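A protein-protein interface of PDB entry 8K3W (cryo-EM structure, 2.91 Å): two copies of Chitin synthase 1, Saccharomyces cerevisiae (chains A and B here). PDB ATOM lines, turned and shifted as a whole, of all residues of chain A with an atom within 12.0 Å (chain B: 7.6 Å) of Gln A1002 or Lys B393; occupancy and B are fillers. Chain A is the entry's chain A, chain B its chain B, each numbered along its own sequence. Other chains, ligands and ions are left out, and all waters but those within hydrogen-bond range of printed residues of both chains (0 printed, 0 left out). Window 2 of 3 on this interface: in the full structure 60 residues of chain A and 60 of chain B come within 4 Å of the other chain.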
ATOM      1  N   LEU A 995      -1.428  22.913   5.020  1.00  0.00           N
ATOM      2  CA  LEU A 995      -2.071  21.701   5.599  1.00  0.00           C
ATOM      3  C   LEU A 995      -3.595  21.831   5.492  1.00  0.00           C
ATOM      4  O   LEU A 995      -4.290  21.374   6.420  1.00  0.00           O
ATOM      5  CB  LEU A 995      -1.632  21.543   7.057  1.00  0.00           C
ATOM      6  N   VAL A 996      -4.087  22.434   4.404  1.00  0.00           N
ATOM      7  CA  VAL A 996      -5.560  22.552   4.184  1.00  0.00           C
ATOM      8  C   VAL A 996      -5.895  21.881   2.849  1.00  0.00           C
ATOM      9  O   VAL A 996      -5.573  22.472   1.799  1.00  0.00           O
ATOM     10  CB  VAL A 996      -6.018  24.023   4.210  1.00  0.00           C
ATOM     11  N   SER A 997      -6.512  20.696   2.888  1.00  0.00           N
ATOM     12  CA  SER A 997      -6.807  19.946   1.638  1.00  0.00           C
ATOM     13  C   SER A 997      -8.257  19.453   1.647  1.00  0.00           C
ATOM     14  O   SER A 997      -8.858  19.411   2.739  1.00  0.00           O
ATOM     15  CB  SER A 997      -5.842  18.802   1.458  1.00  0.00           C
ATOM     16  N   SER A 998      -8.788  19.098   0.474  1.00  0.00           N
ATOM     17  CA  SER A 998     -10.181  18.589   0.379  1.00  0.00           C
ATOM     18  C   SER A 998     -10.164  17.123  -0.064  1.00  0.00           C
ATOM     19  O   SER A 998     -11.118  16.393   0.269  1.00  0.00           O
ATOM     20  CB  SER A 998     -11.001  19.433  -0.559  1.00  0.00           C
ATOM     21  OG  SER A 998     -10.462  19.392  -1.872  1.00  0.00           O
ATOM     22  N   SER A 999      -9.117  16.715  -0.787  1.00  0.00           N
ATOM     23  CA  SER A 999      -9.016  15.313  -1.270  1.00  0.00           C
ATOM     24  C   SER A 999      -8.608  14.400  -0.111  1.00  0.00           C
ATOM     25  O   SER A 999      -9.111  13.261  -0.050  1.00  0.00           O
ATOM     26  CB  SER A 999      -8.047  15.205  -2.415  1.00  0.00           C
ATOM     27  OG  SER A 999      -6.741  15.582  -2.005  1.00  0.00           O
ATOM     28  N   GLU A1000      -7.723  14.884   0.766  1.00  0.00           N
ATOM     29  CA  GLU A1000      -7.285  14.085   1.942  1.00  0.00           C
ATOM     30  C   GLU A1000      -8.502  13.783   2.820  1.00  0.00           C
ATOM     31  O   GLU A1000      -8.548  12.681   3.404  1.00  0.00           O
ATOM     32  CB  GLU A1000      -6.218  14.845   2.732  1.00  0.00           C
ATOM     33  N   ILE A1001      -9.448  14.723   2.902  1.00  0.00           N
ATOM     34  CA  ILE A1001     -10.662  14.535   3.750  1.00  0.00           C
ATOM     35  C   ILE A1001     -11.361  13.243   3.317  1.00  0.00           C
ATOM     36  O   ILE A1001     -11.922  12.555   4.190  1.00  0.00           O
ATOM     37  CB  ILE A1001     -11.596  15.756   3.646  1.00  0.00           C
ATOM     38  N   GLN A1002     -11.314  12.924   2.020  1.00  0.00           N
ATOM     39  CA  GLN A1002     -11.959  11.686   1.507  1.00  0.00           C
ATOM     40  C   GLN A1002     -11.017  10.493   1.704  1.00  0.00           C
ATOM     41  O   GLN A1002     -11.525   9.380   1.945  1.00  0.00           O
ATOM     42  CB  GLN A1002     -12.325  11.843   0.029  1.00  0.00           C
ATOM     43  CG  GLN A1002     -13.733  12.372  -0.200  1.00  0.00           C
ATOM     44  CD  GLN A1002     -14.786  11.305  -0.017  1.00  0.00           C
ATOM     45  OE1 GLN A1002     -15.960  11.512  -0.311  1.00  0.00           O
ATOM     46  NE2 GLN A1002     -14.370  10.145   0.461  1.00  0.00           N
ATOM     47  N   ALA A1003      -9.704  10.719   1.613  1.00  0.00           N
ATOM     48  CA  ALA A1003      -8.732   9.604   1.712  1.00  0.00           C
ATOM     49  C   ALA A1003      -8.891   8.879   3.051  1.00  0.00           C
ATOM     50  O   ALA A1003      -9.056   7.644   3.038  1.00  0.00           O
ATOM     51  CB  ALA A1003      -7.331  10.135   1.544  1.00  0.00           C
ATOM     52  N   ASN A1004      -8.857   9.623   4.161  1.00  0.00           N
ATOM     53  CA  ASN A1004      -8.944   8.989   5.504  1.00  0.00           C
ATOM     54  C   ASN A1004     -10.252   8.200   5.592  1.00  0.00           C
ATOM     55  O   ASN A1004     -10.215   7.047   6.059  1.00  0.00           O
ATOM     56  CB  ASN A1004      -8.839  10.015   6.633  1.00  0.00           C
ATOM     57  CG  ASN A1004      -7.446  10.585   6.789  1.00  0.00           C
ATOM     58  OD1 ASN A1004      -7.203  11.412   7.667  1.00  0.00           O
ATOM     59  ND2 ASN A1004      -6.523  10.147   5.950  1.00  0.00           N
ATOM     60  N   TYR A1005     -11.357   8.798   5.141  1.00  0.00           N
ATOM     61  CA  TYR A1005     -12.679   8.127   5.242  1.00  0.00           C
ATOM     62  C   TYR A1005     -12.633   6.809   4.463  1.00  0.00           C
ATOM     63  O   TYR A1005     -13.065   5.778   5.008  1.00  0.00           O
ATOM     64  CB  TYR A1005     -13.784   9.047   4.722  1.00  0.00           C
ATOM     65  CG  TYR A1005     -15.187   8.528   4.909  1.00  0.00           C
ATOM     66  CD1 TYR A1005     -15.934   8.084   3.833  1.00  0.00           C
ATOM     67  CD2 TYR A1005     -15.772   8.487   6.165  1.00  0.00           C
ATOM     68  CE1 TYR A1005     -17.227   7.615   3.995  1.00  0.00           C
ATOM     69  CE2 TYR A1005     -17.062   8.016   6.346  1.00  0.00           C
ATOM     70  CZ  TYR A1005     -17.792   7.577   5.256  1.00  0.00           C
ATOM     71  OH  TYR A1005     -19.064   7.111   5.424  1.00  0.00           O
ATOM     72  N   ASP A1006     -12.099   6.844   3.240  1.00  0.00           N
ATOM     73  CA  ASP A1006     -12.042   5.620   2.398  1.00  0.00           C
ATOM     74  C   ASP A1006     -11.204   4.553   3.113  1.00  0.00           C
ATOM     75  O   ASP A1006     -11.673   3.402   3.205  1.00  0.00           O
ATOM     76  CB  ASP A1006     -11.495   5.929   1.002  1.00  0.00           C
ATOM     77  N   LYS A1007     -10.022   4.932   3.610  1.00  0.00           N
ATOM     78  CA  LYS A1007      -9.124   3.957   4.288  1.00  0.00           C
ATOM     79  C   LYS A1007      -9.829   3.401   5.527  1.00  0.00           C
ATOM     80  O   LYS A1007      -9.824   2.169   5.707  1.00  0.00           O
ATOM     81  CB  LYS A1007      -7.803   4.627   4.676  1.00  0.00           C
ATOM     82  N   TYR A1008     -10.423   4.281   6.337  1.00  0.00           N
ATOM     83  CA  TYR A1008     -11.109   3.844   7.580  1.00  0.00           C
ATOM     84  C   TYR A1008     -12.240   2.874   7.220  1.00  0.00           C
ATOM     85  O   TYR A1008     -12.391   1.844   7.905  1.00  0.00           O
ATOM     86  CB  TYR A1008     -11.618   5.058   8.361  1.00  0.00           C
ATOM     87  CG  TYR A1008     -10.618   5.641   9.325  1.00  0.00           C
ATOM     88  CD1 TYR A1008      -9.975   4.838  10.251  1.00  0.00           C
ATOM     89  CD2 TYR A1008     -10.324   6.995   9.326  1.00  0.00           C
ATOM     90  CE1 TYR A1008      -9.058   5.359  11.147  1.00  0.00           C
ATOM     91  CE2 TYR A1008      -9.411   7.534  10.217  1.00  0.00           C
ATOM     92  CZ  TYR A1008      -8.775   6.713  11.130  1.00  0.00           C
ATOM     93  OH  TYR A1008      -7.874   7.231  12.013  1.00  0.00           O
ATOM     94  N   LEU A1009     -12.995   3.192   6.165  1.00  0.00           N
ATOM     95  CA  LEU A1009     -14.101   2.306   5.718  1.00  0.00           C
ATOM     96  C   LEU A1009     -13.520   0.949   5.306  1.00  0.00           C
ATOM     97  O   LEU A1009     -14.156  -0.077   5.609  1.00  0.00           O
ATOM     98  CB  LEU A1009     -14.822   2.973   4.545  1.00  0.00           C
ATOM     99  CG  LEU A1009     -16.046   2.224   4.018  1.00  0.00           C
ATOM    100  CD1 LEU A1009     -17.046   1.974   5.135  1.00  0.00           C
ATOM    101  CD2 LEU A1009     -16.697   2.992   2.878  1.00  0.00           C
ATOM    102  N   LYS A1010     -12.358   0.950   4.644  1.00  0.00           N
ATOM    103  CA  LYS A1010     -11.712  -0.317   4.210  1.00  0.00           C
ATOM    104  C   LYS A1010     -11.400  -1.165   5.447  1.00  0.00           C
ATOM    105  O   LYS A1010     -11.605  -2.391   5.388  1.00  0.00           O
ATOM    106  CB  LYS A1010     -10.441  -0.023   3.405  1.00  0.00           C
ATOM    107  N   VAL A1011     -10.924  -0.531   6.522  1.00  0.00           N
ATOM    108  CA  VAL A1011     -10.642  -1.269   7.790  1.00  0.00           C
ATOM    109  C   VAL A1011     -11.954  -1.869   8.302  1.00  0.00           C
ATOM    110  O   VAL A1011     -11.927  -3.015   8.784  1.00  0.00           O
ATOM    111  CB  VAL A1011      -9.996  -0.348   8.842  1.00  0.00           C
ATOM    112  CG1 VAL A1011      -9.690  -1.092  10.133  1.00  0.00           C
ATOM    113  CG2 VAL A1011      -8.748   0.334   8.304  1.00  0.00           C
ATOM    114  N   PRO B 390     -14.897  19.743   7.781  1.00  0.00           N
ATOM    115  CA  PRO B 390     -16.113  19.105   7.281  1.00  0.00           C
ATOM    116  C   PRO B 390     -15.880  17.597   7.157  1.00  0.00           C
ATOM    117  O   PRO B 390     -14.762  17.181   6.903  1.00  0.00           O
ATOM    118  CB  PRO B 390     -16.411  19.820   5.950  1.00  0.00           C
ATOM    119  CG  PRO B 390     -15.114  20.524   5.605  1.00  0.00           C
ATOM    120  CD  PRO B 390     -14.482  20.867   6.938  1.00  0.00           C
ATOM    121  N   ILE B 391     -16.942  16.823   7.360  1.00  0.00           N
ATOM    122  CA  ILE B 391     -16.817  15.343   7.306  1.00  0.00           C
ATOM    123  C   ILE B 391     -16.559  14.947   5.850  1.00  0.00           C
ATOM    124  O   ILE B 391     -16.613  15.836   4.982  1.00  0.00           O
ATOM    125  CB  ILE B 391     -18.088  14.721   7.902  1.00  0.00           C
ATOM    126  CG1 ILE B 391     -19.275  15.681   7.800  1.00  0.00           C
ATOM    127  CG2 ILE B 391     -17.841  14.283   9.336  1.00  0.00           C
ATOM    128  CD1 ILE B 391     -20.621  15.005   7.872  1.00  0.00           C
ATOM    129  N   SER B 392     -16.273  13.667   5.597  1.00  0.00           N
ATOM    130  CA  SER B 392     -15.952  13.181   4.230  1.00  0.00           C
ATOM    131  C   SER B 392     -17.038  13.582   3.236  1.00  0.00           C
ATOM    132  O   SER B 392     -18.219  13.503   3.600  1.00  0.00           O
ATOM    133  CB  SER B 392     -15.786  11.697   4.240  1.00  0.00           C
ATOM    134  OG  SER B 392     -17.023  11.055   4.496  1.00  0.00           O
ATOM    135  N   LYS B 393     -16.646  13.948   2.017  1.00  0.00           N
ATOM    136  CA  LYS B 393     -17.655  14.275   0.980  1.00  0.00           C
ATOM    137  C   LYS B 393     -18.655  13.120   0.913  1.00  0.00           C
ATOM    138  O   LYS B 393     -19.869  13.400   0.834  1.00  0.00           O
ATOM    139  CB  LYS B 393     -16.971  14.493  -0.370  1.00  0.00           C
ATOM    140  N   THR B 394     -18.164  11.877   0.965  1.00  0.00           N
ATOM    141  CA  THR B 394     -19.048  10.679   0.941  1.00  0.00           C
ATOM    142  C   THR B 394     -20.092  10.776   2.057  1.00  0.00           C
ATOM    143  O   THR B 394     -21.295  10.752   1.739  1.00  0.00           O
ATOM    144  CB  THR B 394     -18.229   9.394   1.092  1.00  0.00           C
ATOM    145  OG1 THR B 394     -16.936   9.737   1.593  1.00  0.00           O
ATOM    146  CG2 THR B 394     -18.088   8.630  -0.206  1.00  0.00           C
ATOM    147  N   LEU B 395     -19.643  10.848   3.314  1.00  0.00           N
ATOM    148  CA  LEU B 395     -20.570  10.989   4.467  1.00  0.00           C
ATOM    149  C   LEU B 395     -21.523  12.152   4.196  1.00  0.00           C
ATOM    150  O   LEU B 395     -22.748  11.925   4.199  1.00  0.00           O
ATOM    151  CB  LEU B 395     -19.747  11.270   5.726  1.00  0.00           C
ATOM    152  CG  LEU B 395     -19.832  10.212   6.822  1.00  0.00           C
ATOM    153  CD1 LEU B 395     -19.836  10.864   8.195  1.00  0.00           C
ATOM    154  CD2 LEU B 395     -21.066   9.340   6.640  1.00  0.00           C
ATOM    155  N   LEU B 396     -20.973  13.347   3.971  1.00  0.00           N
ATOM    156  CA  LEU B 396     -21.818  14.550   3.759  1.00  0.00           C
ATOM    157  C   LEU B 396     -22.794  14.285   2.609  1.00  0.00           C
ATOM    158  O   LEU B 396     -23.912  14.833   2.647  1.00  0.00           O
ATOM    159  CB  LEU B 396     -20.915  15.746   3.445  1.00  0.00           C
ATOM    160  CG  LEU B 396     -21.192  17.009   4.257  1.00  0.00           C
ATOM    161  CD1 LEU B 396     -22.288  16.762   5.282  1.00  0.00           C
ATOM    162  CD2 LEU B 396     -19.924  17.505   4.934  1.00  0.00           C
ATOM    163  N   ASP B 397     -22.380  13.481   1.628  1.00  0.00           N
ATOM    164  CA  ASP B 397     -23.252  13.185   0.461  1.00  0.00           C
ATOM    165  C   ASP B 397     -24.542  12.522   0.951  1.00  0.00           C
ATOM    166  O   ASP B 397     -25.628  13.008   0.583  1.00  0.00           O
ATOM    167  CB  ASP B 397     -22.530  12.310  -0.563  1.00  0.00           C
ATOM    168  N   GLN B 398     -24.423  11.461   1.756  1.00  0.00           N
ATOM    169  CA  GLN B 398     -25.619  10.723   2.244  1.00  0.00           C
ATOM    170  C   GLN B 398     -26.351  11.564   3.296  1.00  0.00           C
ATOM    171  O   GLN B 398     -27.593  11.512   3.322  1.00  0.00           O
ATOM    172  CB  GLN B 398     -25.236   9.348   2.800  1.00  0.00           C
ATOM    173  CG  GLN B 398     -23.743   9.171   3.032  1.00  0.00           C
ATOM    174  CD  GLN B 398     -23.405   7.775   3.494  1.00  0.00           C
ATOM    175  OE1 GLN B 398     -24.281   6.932   3.670  1.00  0.00           O
ATOM    176  NE2 GLN B 398     -22.124   7.521   3.694  1.00  0.00           N
ATOM    177  N   TYR B 399     -25.617  12.297   4.140  1.00  0.00           N
ATOM    178  CA  TYR B 399     -26.291  13.062   5.220  1.00  0.00           C
ATOM    179  C   TYR B 399     -27.358  13.944   4.575  1.00  0.00           C
ATOM    180  O   TYR B 399     -28.491  13.982   5.080  1.00  0.00           O
ATOM    181  CB  TYR B 399     -25.298  13.922   6.002  1.00  0.00           C
ATOM    182  CG  TYR B 399     -24.513  13.202   7.069  1.00  0.00           C
ATOM    183  CD1 TYR B 399     -24.311  11.834   7.011  1.00  0.00           C
ATOM    184  CD2 TYR B 399     -23.960  13.896   8.131  1.00  0.00           C
ATOM    185  CE1 TYR B 399     -23.584  11.171   7.986  1.00  0.00           C
ATOM    186  CE2 TYR B 399     -23.231  13.249   9.114  1.00  0.00           C
ATOM    187  CZ  TYR B 399     -23.043  11.883   9.041  1.00  0.00           C
ATOM    188  OH  TYR B 399     -22.321  11.244  10.004  1.00  0.00           O
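The backbone NH (N) of Thr B394 lies within hydrogen-bond range of the side-chain amide oxygen (OE1) of Gln A1002, 2.6 Å away. The backbone NH of Lys B393 lies close to the side-chain amide oxygen of Gln A1002, at 3.4 Å.
Printed residues of chain A that touch a printed residue of chain B: Ile A1001, Gln A1002 and Tyr A1005. Hydrophobic or aromatic side chains of chain A within 4 Å of the printed part of chain B: Tyr A1005. Along chain B the printed residues that touch a printed residue of chain A span positions 392 to 398. Among the printed residues, 7 pairs touch across the chains.
The side-chain hydroxyl of Ser B392 is in hydrogen-bond range of the side-chain hydroxyl of Thr B394 (3.2 Å). N of Leu B395 is in hydrogen-bond range of OG of Ser B392, 2.9 Å away.
No position is printed for both chains.
Gln A1002 touches just these residues of chain B: Lys B393 (3.1 Å) and Thr B394 (2.6 Å). Lys B393 touches just one residue of chain A: Gln A1002. Ile B391 touches none of the printed residues of chain A. Ser B392 touches just these residues of chain A: Ile A1001 and Tyr A1005. Of the printed residues of chain A, Thr B394 touches Gln A1002 and Tyr A1005. No residue of chain A comes within 4 Å of Asp B397. Of the printed residues of chain B, Tyr A1005 touches Ser B392, Thr B394, Leu B395 and Gln B398. Printed residues of chain A within 4 Å of Gln B398: Tyr A1005 (3.5 Å). Pro B390 touches none of the printed residues of chain A. Ala A1003 touches none of the printed residues of chain B. The nearest residue of chain A that does not touch Lys B393 is Ile A1001 (5.4 Å).
Among the printed residues, merely in contact across the chains: Ile A1001 with Ser B392, Tyr A1005 with Ser B392, Tyr A1005 with Thr B394, Tyr A1005 with Leu B395 and Tyr A1005 with Gln B398.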
